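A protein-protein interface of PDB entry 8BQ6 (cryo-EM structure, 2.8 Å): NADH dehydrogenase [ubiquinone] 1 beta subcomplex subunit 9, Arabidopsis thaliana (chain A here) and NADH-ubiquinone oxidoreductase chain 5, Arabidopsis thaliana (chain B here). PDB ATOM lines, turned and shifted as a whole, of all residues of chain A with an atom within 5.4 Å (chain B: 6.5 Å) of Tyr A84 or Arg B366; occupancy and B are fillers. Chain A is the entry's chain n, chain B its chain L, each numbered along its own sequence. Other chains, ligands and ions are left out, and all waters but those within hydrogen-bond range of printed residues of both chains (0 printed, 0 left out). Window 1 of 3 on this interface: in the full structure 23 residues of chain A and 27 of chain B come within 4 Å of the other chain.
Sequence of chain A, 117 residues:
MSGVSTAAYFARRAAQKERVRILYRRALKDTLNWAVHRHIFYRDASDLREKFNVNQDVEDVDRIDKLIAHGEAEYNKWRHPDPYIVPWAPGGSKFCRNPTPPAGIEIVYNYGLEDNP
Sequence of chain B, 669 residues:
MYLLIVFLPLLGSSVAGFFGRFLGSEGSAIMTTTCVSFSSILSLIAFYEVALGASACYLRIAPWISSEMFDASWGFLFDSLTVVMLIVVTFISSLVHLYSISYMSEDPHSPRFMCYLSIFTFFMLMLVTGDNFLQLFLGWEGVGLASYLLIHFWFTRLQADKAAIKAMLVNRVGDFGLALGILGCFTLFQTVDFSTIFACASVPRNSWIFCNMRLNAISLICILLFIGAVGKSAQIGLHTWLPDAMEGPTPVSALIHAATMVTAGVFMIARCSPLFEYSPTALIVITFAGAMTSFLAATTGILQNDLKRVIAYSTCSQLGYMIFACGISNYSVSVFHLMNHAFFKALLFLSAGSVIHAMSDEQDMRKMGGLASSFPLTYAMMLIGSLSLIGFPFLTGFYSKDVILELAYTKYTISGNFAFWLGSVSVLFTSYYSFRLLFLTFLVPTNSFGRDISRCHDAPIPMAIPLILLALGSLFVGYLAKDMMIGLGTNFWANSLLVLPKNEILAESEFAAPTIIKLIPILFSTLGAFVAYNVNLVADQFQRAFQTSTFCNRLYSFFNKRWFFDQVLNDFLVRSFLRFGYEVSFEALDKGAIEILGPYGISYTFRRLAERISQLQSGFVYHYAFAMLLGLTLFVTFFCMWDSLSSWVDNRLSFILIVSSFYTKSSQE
OH of Tyr A84 is in hydrogen-bond range of OE1 of Glu B362 (2.9 Å). NH1 of Arg B366 lies close to NE2 of His A80, at 3.5 Å. The side-chain carboxylate (OD1) of Asp A82 lies within salt-bridge range of the guanidinium group (NH2) of Arg B366, at 3.99 Å. O of Val A36 sits at hydrogen-bond distance from ND2 of Asn B447 (3.1 Å).
O of Asn B305 is in hydrogen-bond range of N of Met B365 (2.6 Å). The side-chain amide nitrogen (ND2) of Asn B305 lies close to the guanidinium group (NH2) of Arg B436 (3.4 Å). The side-chain carboxylate (OD1) of Asp B364 is in salt-bridge range of the guanidinium group (NE) of Arg B366 (2.7 Å). O of Asn A33 sits close to NE2 of His A80. The backbone NH (N) of Tyr A84 lies within hydrogen-bond range of the side-chain amide oxygen (OD1) of Asn A33 (3.0 Å). ND1 of His A80 lies within hydrogen-bond range of N of Asp A82 (2.9 Å).
Among the printed residues, pairs that only touch across the chains: Asn A33 with Arg B366 (3.7 Å), Val A36 with Arg B366 (3.8 Å), Asp A82 with Asn B305 (3.6 Å), Pro A83 with Arg B366 (3.8 Å), Tyr A84 with Asp B364 (3.8 Å), Tyr A84 with Arg B366 (3.8 Å), Tyr A84 with Lys B367 (3.3 Å) and Tyr A84 with Phe B449 (3.3 Å).
Of the printed residues of chain B, His A80 touches Arg B366. Tyr A84 touches just these residues of chain B: Glu B362 (2.9 Å), Asp B364 (3.8 Å), Arg B366 (3.8 Å), Lys B367 (3.3 Å) and Phe B449 (3.3 Å). Of the printed residues of chain A, Glu B362 touches Tyr A84. Of chain A, only Asn A33 (3.7 Å), Val A36 (3.8 Å), His A80 (3.4 Å), Asp A82 (2.7 Å), Pro A83 (3.8 Å) and Tyr A84 (3.8 Å) come within 4 Å of Arg B366. Printed residues of chain A within 4 Å of Asn B447: Val A36 (3.1 Å). The nearest printed residue of chain A that does not touch Arg B366 is Ile A85 (5.9 Å).
Printed residues of chain A that touch a printed residue of chain B: Asn A33, Val A36, His A80, Asp A82, Pro A83 and Tyr A84. Hydrophobic or aromatic side chains of chain A that line the printed part of chain B: Val A36, His A80 and Tyr A84. Hydrophobic or aromatic side chains of chain B within 4 Å of the printed part of chain A: Phe B449. Among the printed residues, Asp or Glu carboxylates within 4 Å of a Lys or Arg side-chain nitrogen of the other chain: Asp A82 with Arg B366 (3.99 Å).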
ATOM      1  N   ASN A  33      23.515   0.285   7.560  1.00  0.00           N
ATOM      2  CA  ASN A  33      24.181   1.584   7.617  1.00  0.00           C
ATOM      3  C   ASN A  33      24.732   1.866   9.006  1.00  0.00           C
ATOM      4  O   ASN A  33      25.818   2.438   9.147  1.00  0.00           O
ATOM      5  CB  ASN A  33      23.220   2.700   7.212  1.00  0.00           C
ATOM      6  CG  ASN A  33      23.029   2.787   5.723  1.00  0.00           C
ATOM      7  OD1 ASN A  33      23.980   2.645   4.957  1.00  0.00           O
ATOM      8  ND2 ASN A  33      21.796   3.030   5.299  1.00  0.00           N
ATOM      9  N   VAL A  36      27.716  -1.295   9.710  1.00  0.00           N
ATOM     10  CA  VAL A  36      28.925  -1.306   8.890  1.00  0.00           C
ATOM     11  C   VAL A  36      29.434  -2.732   8.727  1.00  0.00           C
ATOM     12  O   VAL A  36      29.432  -3.280   7.620  1.00  0.00           O
ATOM     13  CB  VAL A  36      30.023  -0.398   9.477  1.00  0.00           C
ATOM     14  CG1 VAL A  36      31.262  -0.436   8.599  1.00  0.00           C
ATOM     15  CG2 VAL A  36      29.516   1.025   9.634  1.00  0.00           C
ATOM     16  N   HIS A  80      19.376   6.529   9.446  1.00  0.00           N
ATOM     17  CA  HIS A  80      20.780   6.922   9.387  1.00  0.00           C
ATOM     18  C   HIS A  80      20.933   8.221   8.603  1.00  0.00           C
ATOM     19  O   HIS A  80      20.442   8.319   7.474  1.00  0.00           O
ATOM     20  CB  HIS A  80      21.625   5.822   8.753  1.00  0.00           C
ATOM     21  CG  HIS A  80      23.090   5.956   9.027  1.00  0.00           C
ATOM     22  ND1 HIS A  80      23.845   7.000   8.541  1.00  0.00           N
ATOM     23  CD2 HIS A  80      23.936   5.185   9.751  1.00  0.00           C
ATOM     24  CE1 HIS A  80      25.095   6.864   8.945  1.00  0.00           C
ATOM     25  NE2 HIS A  80      25.177   5.770   9.680  1.00  0.00           N
ATOM     26  N   ASP A  82      23.399   9.427   7.018  1.00  0.00           N
ATOM     27  CA  ASP A  82      24.228   9.256   5.825  1.00  0.00           C
ATOM     28  C   ASP A  82      24.078   7.832   5.314  1.00  0.00           C
ATOM     29  O   ASP A  82      24.944   6.978   5.552  1.00  0.00           O
ATOM     30  CB  ASP A  82      25.693   9.582   6.115  1.00  0.00           C
ATOM     31  CG  ASP A  82      26.428  10.067   4.889  1.00  0.00           C
ATOM     32  OD1 ASP A  82      27.629   9.755   4.755  1.00  0.00           O
ATOM     33  OD2 ASP A  82      25.800  10.756   4.056  1.00  0.00           O
ATOM     34  N   PRO A  83      22.988   7.535   4.612  1.00  0.00           N
ATOM     35  CA  PRO A  83      22.800   6.181   4.088  1.00  0.00           C
ATOM     36  C   PRO A  83      23.734   5.883   2.928  1.00  0.00           C
ATOM     37  O   PRO A  83      24.234   6.781   2.247  1.00  0.00           O
ATOM     38  CB  PRO A  83      21.338   6.180   3.632  1.00  0.00           C
ATOM     39  CG  PRO A  83      21.052   7.594   3.325  1.00  0.00           C
ATOM     40  CD  PRO A  83      21.833   8.402   4.321  1.00  0.00           C
ATOM     41  N   TYR A  84      23.965   4.593   2.714  1.00  0.00           N
ATOM     42  CA  TYR A  84      24.795   4.162   1.604  1.00  0.00           C
ATOM     43  C   TYR A  84      23.999   4.189   0.308  1.00  0.00           C
ATOM     44  O   TYR A  84      22.816   3.839   0.279  1.00  0.00           O
ATOM     45  CB  TYR A  84      25.327   2.754   1.852  1.00  0.00           C
ATOM     46  CG  TYR A  84      25.984   2.179   0.634  1.00  0.00           C
ATOM     47  CD1 TYR A  84      27.254   2.583   0.260  1.00  0.00           C
ATOM     48  CD2 TYR A  84      25.321   1.269  -0.173  1.00  0.00           C
ATOM     49  CE1 TYR A  84      27.853   2.080  -0.865  1.00  0.00           C
ATOM     50  CE2 TYR A  84      25.912   0.762  -1.299  1.00  0.00           C
ATOM     51  CZ  TYR A  84      27.181   1.168  -1.638  1.00  0.00           C
ATOM     52  OH  TYR A  84      27.781   0.665  -2.764  1.00  0.00           O
ATOM     53  N   ILE A  85      24.650   4.607  -0.772  1.00  0.00           N
ATOM     54  CA  ILE A  85      24.034   4.633  -2.090  1.00  0.00           C
ATOM     55  C   ILE A  85      25.003   4.015  -3.082  1.00  0.00           C
ATOM     56  O   ILE A  85      26.194   4.348  -3.080  1.00  0.00           O
ATOM     57  CB  ILE A  85      23.663   6.064  -2.524  1.00  0.00           C
ATOM     58  CG1 ILE A  85      22.803   6.727  -1.454  1.00  0.00           C
ATOM     59  CG2 ILE A  85      22.908   6.041  -3.839  1.00  0.00           C
ATOM     60  CD1 ILE A  85      23.175   8.152  -1.190  1.00  0.00           C
ATOM     61  N   VAL A  86      24.499   3.112  -3.913  1.00  0.00           N
ATOM     62  CA  VAL A  86      25.301   2.639  -5.044  1.00  0.00           C
ATOM     63  C   VAL A  86      25.676   3.843  -5.899  1.00  0.00           C
ATOM     64  O   VAL A  86      24.807   4.689  -6.185  1.00  0.00           O
ATOM     65  CB  VAL A  86      24.515   1.602  -5.863  1.00  0.00           C
ATOM     66  CG1 VAL A  86      25.402   0.968  -6.901  1.00  0.00           C
ATOM     67  CG2 VAL A  86      23.921   0.544  -4.954  1.00  0.00           C
ATOM     68  N   PRO A  87      26.939   3.995  -6.305  1.00  0.00           N
ATOM     69  CA  PRO A  87      27.357   5.260  -6.933  1.00  0.00           C
ATOM     70  C   PRO A  87      26.574   5.644  -8.178  1.00  0.00           C
ATOM     71  O   PRO A  87      26.320   6.838  -8.379  1.00  0.00           O
ATOM     72  CB  PRO A  87      28.838   5.014  -7.245  1.00  0.00           C
ATOM     73  CG  PRO A  87      29.264   4.031  -6.214  1.00  0.00           C
ATOM     74  CD  PRO A  87      28.088   3.129  -5.992  1.00  0.00           C
ATOM     75  N   ASN B 305      31.859   8.990   6.095  1.00  0.00           N
ATOM     76  CA  ASN B 305      31.999   7.669   5.505  1.00  0.00           C
ATOM     77  C   ASN B 305      32.622   7.688   4.121  1.00  0.00           C
ATOM     78  O   ASN B 305      32.987   6.625   3.610  1.00  0.00           O
ATOM     79  CB  ASN B 305      30.636   6.970   5.440  1.00  0.00           C
ATOM     80  CG  ASN B 305      30.023   6.791   6.806  1.00  0.00           C
ATOM     81  OD1 ASN B 305      28.924   7.272   7.077  1.00  0.00           O
ATOM     82  ND2 ASN B 305      30.750   6.120   7.690  1.00  0.00           N
ATOM     83  N   ASP B 306      32.768   8.860   3.514  1.00  0.00           N
ATOM     84  CA  ASP B 306      33.329   8.985   2.180  1.00  0.00           C
ATOM     85  C   ASP B 306      34.816   9.303   2.288  1.00  0.00           C
ATOM     86  O   ASP B 306      35.220  10.135   3.106  1.00  0.00           O
ATOM     87  CB  ASP B 306      32.568  10.065   1.403  1.00  0.00           C
ATOM     88  CG  ASP B 306      33.108  10.288   0.005  1.00  0.00           C
ATOM     89  OD1 ASP B 306      34.192  10.888  -0.128  1.00  0.00           O
ATOM     90  OD2 ASP B 306      32.441   9.871  -0.966  1.00  0.00           O
ATOM     91  N   GLU B 362      33.898   3.344  -6.142  1.00  0.00           N
ATOM     92  CA  GLU B 362      33.316   3.290  -4.809  1.00  0.00           C
ATOM     93  C   GLU B 362      34.061   4.251  -3.894  1.00  0.00           C
ATOM     94  O   GLU B 362      35.293   4.333  -3.935  1.00  0.00           O
ATOM     95  CB  GLU B 362      33.385   1.867  -4.255  1.00  0.00           C
ATOM     96  CG  GLU B 362      32.828   1.724  -2.848  1.00  0.00           C
ATOM     97  CD  GLU B 362      31.320   1.849  -2.799  1.00  0.00           C
ATOM     98  OE1 GLU B 362      30.633   0.871  -3.155  1.00  0.00           O
ATOM     99  OE2 GLU B 362      30.822   2.926  -2.412  1.00  0.00           O
ATOM    100  N   GLN B 363      33.318   4.988  -3.071  1.00  0.00           N
ATOM    101  CA  GLN B 363      33.910   5.970  -2.177  1.00  0.00           C
ATOM    102  C   GLN B 363      33.470   5.833  -0.730  1.00  0.00           C
ATOM    103  O   GLN B 363      34.036   6.513   0.133  1.00  0.00           O
ATOM    104  CB  GLN B 363      33.586   7.393  -2.648  1.00  0.00           C
ATOM    105  CG  GLN B 363      34.497   7.905  -3.730  1.00  0.00           C
ATOM    106  CD  GLN B 363      33.902   9.078  -4.467  1.00  0.00           C
ATOM    107  OE1 GLN B 363      33.785   9.062  -5.691  1.00  0.00           O
ATOM    108  NE2 GLN B 363      33.515  10.105  -3.724  1.00  0.00           N
ATOM    109  N   ASP B 364      32.483   4.995  -0.442  1.00  0.00           N
ATOM    110  CA  ASP B 364      32.000   4.793   0.915  1.00  0.00           C
ATOM    111  C   ASP B 364      32.908   3.796   1.622  1.00  0.00           C
ATOM    112  O   ASP B 364      33.115   2.682   1.129  1.00  0.00           O
ATOM    113  CB  ASP B 364      30.560   4.289   0.890  1.00  0.00           C
ATOM    114  CG  ASP B 364      29.764   4.759   2.077  1.00  0.00           C
ATOM    115  OD1 ASP B 364      29.936   4.182   3.168  1.00  0.00           O
ATOM    116  OD2 ASP B 364      28.965   5.704   1.920  1.00  0.00           O
ATOM    117  N   MET B 365      33.448   4.192   2.776  1.00  0.00           N
ATOM    118  CA  MET B 365      34.360   3.310   3.494  1.00  0.00           C
ATOM    119  C   MET B 365      33.646   2.116   4.112  1.00  0.00           C
ATOM    120  O   MET B 365      34.298   1.112   4.417  1.00  0.00           O
ATOM    121  CB  MET B 365      35.109   4.086   4.578  1.00  0.00           C
ATOM    122  CG  MET B 365      36.206   4.979   4.033  1.00  0.00           C
ATOM    123  SD  MET B 365      37.208   5.752   5.312  1.00  0.00           S
ATOM    124  CE  MET B 365      36.017   6.857   6.061  1.00  0.00           C
ATOM    125  N   ARG B 366      32.330   2.196   4.294  1.00  0.00           N
ATOM    126  CA  ARG B 366      31.592   1.072   4.852  1.00  0.00           C
ATOM    127  C   ARG B 366      31.472  -0.094   3.882  1.00  0.00           C
ATOM    128  O   ARG B 366      31.070  -1.184   4.302  1.00  0.00           O
ATOM    129  CB  ARG B 366      30.204   1.525   5.293  1.00  0.00           C
ATOM    130  CG  ARG B 366      30.212   2.696   6.249  1.00  0.00           C
ATOM    131  CD  ARG B 366      28.802   3.202   6.466  1.00  0.00           C
ATOM    132  NE  ARG B 366      28.393   4.108   5.401  1.00  0.00           N
ATOM    133  CZ  ARG B 366      27.400   4.981   5.504  1.00  0.00           C
ATOM    134  NH1 ARG B 366      26.651   5.050   6.590  1.00  0.00           N
ATOM    135  NH2 ARG B 366      27.151   5.801   4.486  1.00  0.00           N
ATOM    136  N   LYS B 367      31.795   0.103   2.609  1.00  0.00           N
ATOM    137  CA  LYS B 367      31.831  -0.970   1.625  1.00  0.00           C
ATOM    138  C   LYS B 367      33.251  -1.194   1.126  1.00  0.00           C
ATOM    139  O   LYS B 367      33.487  -1.400  -0.065  1.00  0.00           O
ATOM    140  CB  LYS B 367      30.889  -0.681   0.461  1.00  0.00           C
ATOM    141  CG  LYS B 367      29.516  -0.227   0.900  1.00  0.00           C
ATOM    142  CD  LYS B 367      28.731  -1.331   1.587  1.00  0.00           C
ATOM    143  CE  LYS B 367      27.339  -0.835   1.941  1.00  0.00           C
ATOM    144  NZ  LYS B 367      26.312  -1.906   2.059  1.00  0.00           N
ATOM    145  N   MET B 368      34.216  -1.128   2.036  1.00  0.00           N
ATOM    146  CA  MET B 368      35.605  -1.440   1.726  1.00  0.00           C
ATOM    147  C   MET B 368      36.121  -2.337   2.849  1.00  0.00           C
ATOM    148  O   MET B 368      35.368  -2.790   3.720  1.00  0.00           O
ATOM    149  CB  MET B 368      36.438  -0.161   1.561  1.00  0.00           C
ATOM    150  CG  MET B 368      35.770   0.886   0.689  1.00  0.00           C
ATOM    151  SD  MET B 368      36.731   2.367   0.346  1.00  0.00           S
ATOM    152  CE  MET B 368      35.917   2.888  -1.160  1.00  0.00           C
ATOM    153  N   ARG B 436      41.121   5.613  11.657  1.00  0.00           N
ATOM    154  CA  ARG B 436      39.792   5.098  11.335  1.00  0.00           C
ATOM    155  C   ARG B 436      39.650   4.847   9.841  1.00  0.00           C
ATOM    156  O   ARG B 436      39.090   3.827   9.424  1.00  0.00           O
ATOM    157  CB  ARG B 436      38.714   6.071  11.812  1.00  0.00           C
ATOM    158  CG  ARG B 436      37.304   5.638  11.455  1.00  0.00           C
ATOM    159  CD  ARG B 436      36.266   6.576  12.029  1.00  0.00           C
ATOM    160  NE  ARG B 436      34.945   6.318  11.467  1.00  0.00           N
ATOM    161  CZ  ARG B 436      34.487   6.876  10.356  1.00  0.00           C
ATOM    162  NH1 ARG B 436      35.236   7.694   9.634  1.00  0.00           N
ATOM    163  NH2 ARG B 436      33.251   6.600   9.952  1.00  0.00           N
ATOM    164  N   LEU B 440      39.133   0.929   8.298  1.00  0.00           N
ATOM    165  CA  LEU B 440      37.931   0.636   7.529  1.00  0.00           C
ATOM    166  C   LEU B 440      38.258   0.306   6.081  1.00  0.00           C
ATOM    167  O   LEU B 440      37.626  -0.569   5.480  1.00  0.00           O
ATOM    168  CB  LEU B 440      36.972   1.818   7.591  1.00  0.00           C
ATOM    169  CG  LEU B 440      36.255   2.015   8.919  1.00  0.00           C
ATOM    170  CD1 LEU B 440      35.361   3.228   8.825  1.00  0.00           C
ATOM    171  CD2 LEU B 440      35.459   0.772   9.266  1.00  0.00           C
ATOM    172  N   ASN B 447      34.060  -5.579   3.756  1.00  0.00           N
ATOM    173  CA  ASN B 447      32.671  -5.164   3.860  1.00  0.00           C
ATOM    174  C   ASN B 447      32.093  -4.819   2.496  1.00  0.00           C
ATOM    175  O   ASN B 447      31.108  -4.082   2.406  1.00  0.00           O
ATOM    176  CB  ASN B 447      32.561  -3.970   4.803  1.00  0.00           C
ATOM    177  CG  ASN B 447      32.373  -4.385   6.239  1.00  0.00           C
ATOM    178  OD1 ASN B 447      32.171  -5.561   6.534  1.00  0.00           O
ATOM    179  ND2 ASN B 447      32.485  -3.426   7.147  1.00  0.00           N
ATOM    180  N   SER B 448      32.687  -5.352   1.436  1.00  0.00           N
ATOM    181  CA  SER B 448      32.502  -4.826   0.098  1.00  0.00           C
ATOM    182  C   SER B 448      31.726  -5.808  -0.779  1.00  0.00           C
ATOM    183  O   SER B 448      31.371  -6.914  -0.364  1.00  0.00           O
ATOM    184  CB  SER B 448      33.867  -4.481  -0.495  1.00  0.00           C
ATOM    185  OG  SER B 448      34.486  -5.617  -1.066  1.00  0.00           O
ATOM    186  N   PHE B 449      31.446  -5.383  -2.010  1.00  0.00           N
ATOM    187  CA  PHE B 449      30.724  -6.195  -2.980  1.00  0.00           C
ATOM    188  C   PHE B 449      31.692  -7.050  -3.786  1.00  0.00           C
ATOM    189  O   PHE B 449      32.812  -6.628  -4.086  1.00  0.00           O
ATOM    190  CB  PHE B 449      29.907  -5.313  -3.926  1.00  0.00           C
ATOM    191  CG  PHE B 449      28.809  -4.551  -3.251  1.00  0.00           C
ATOM    192  CD1 PHE B 449      27.576  -5.135  -3.030  1.00  0.00           C
ATOM    193  CD2 PHE B 449      29.006  -3.245  -2.844  1.00  0.00           C
ATOM    194  CE1 PHE B 449      26.564  -4.432  -2.413  1.00  0.00           C
ATOM    195  CE2 PHE B 449      27.997  -2.541  -2.225  1.00  0.00           C
ATOM    196  CZ  PHE B 449      26.775  -3.136  -2.007  1.00  0.00           C
ATOM    197  N   ASP B 452      33.058  -5.811  -7.294  1.00  0.00           N
ATOM    198  CA  ASP B 452      34.139  -4.834  -7.222  1.00  0.00           C
ATOM    199  C   ASP B 452      35.473  -5.518  -6.955  1.00  0.00           C
ATOM    200  O   ASP B 452      36.493  -5.167  -7.560  1.00  0.00           O
ATOM    201  CB  ASP B 452      33.843  -3.804  -6.131  1.00  0.00           C
ATOM    202  CG  ASP B 452      32.659  -2.911  -6.464  1.00  0.00           C
ATOM    203  OD1 ASP B 452      32.415  -2.638  -7.659  1.00  0.00           O
ATOM    204  OD2 ASP B 452      31.968  -2.477  -5.518  1.00  0.00           O
ATOM    205  N   TYR B 556      25.063  12.285  17.085  1.00  0.00           N
ATOM    206  CA  TYR B 556      25.667  11.656  15.914  1.00  0.00           C
ATOM    207  C   TYR B 556      25.409  12.476  14.661  1.00  0.00           C
ATOM    208  O   TYR B 556      26.295  12.645  13.816  1.00  0.00           O
ATOM    209  CB  TYR B 556      25.109  10.246  15.728  1.00  0.00           C
ATOM    210  CG  TYR B 556      25.955   9.356  14.849  1.00  0.00           C
ATOM    211  CD1 TYR B 556      27.119   8.781  15.328  1.00  0.00           C
ATOM    212  CD2 TYR B 556      25.606   9.119  13.526  1.00  0.00           C
ATOM    213  CE1 TYR B 556      27.894   7.970  14.529  1.00  0.00           C
ATOM    214  CE2 TYR B 556      26.380   8.312  12.717  1.00  0.00           C
ATOM    215  CZ  TYR B 556      27.524   7.741  13.224  1.00  0.00           C
ATOM    216  OH  TYR B 556      28.301   6.934  12.426  1.00  0.00           O
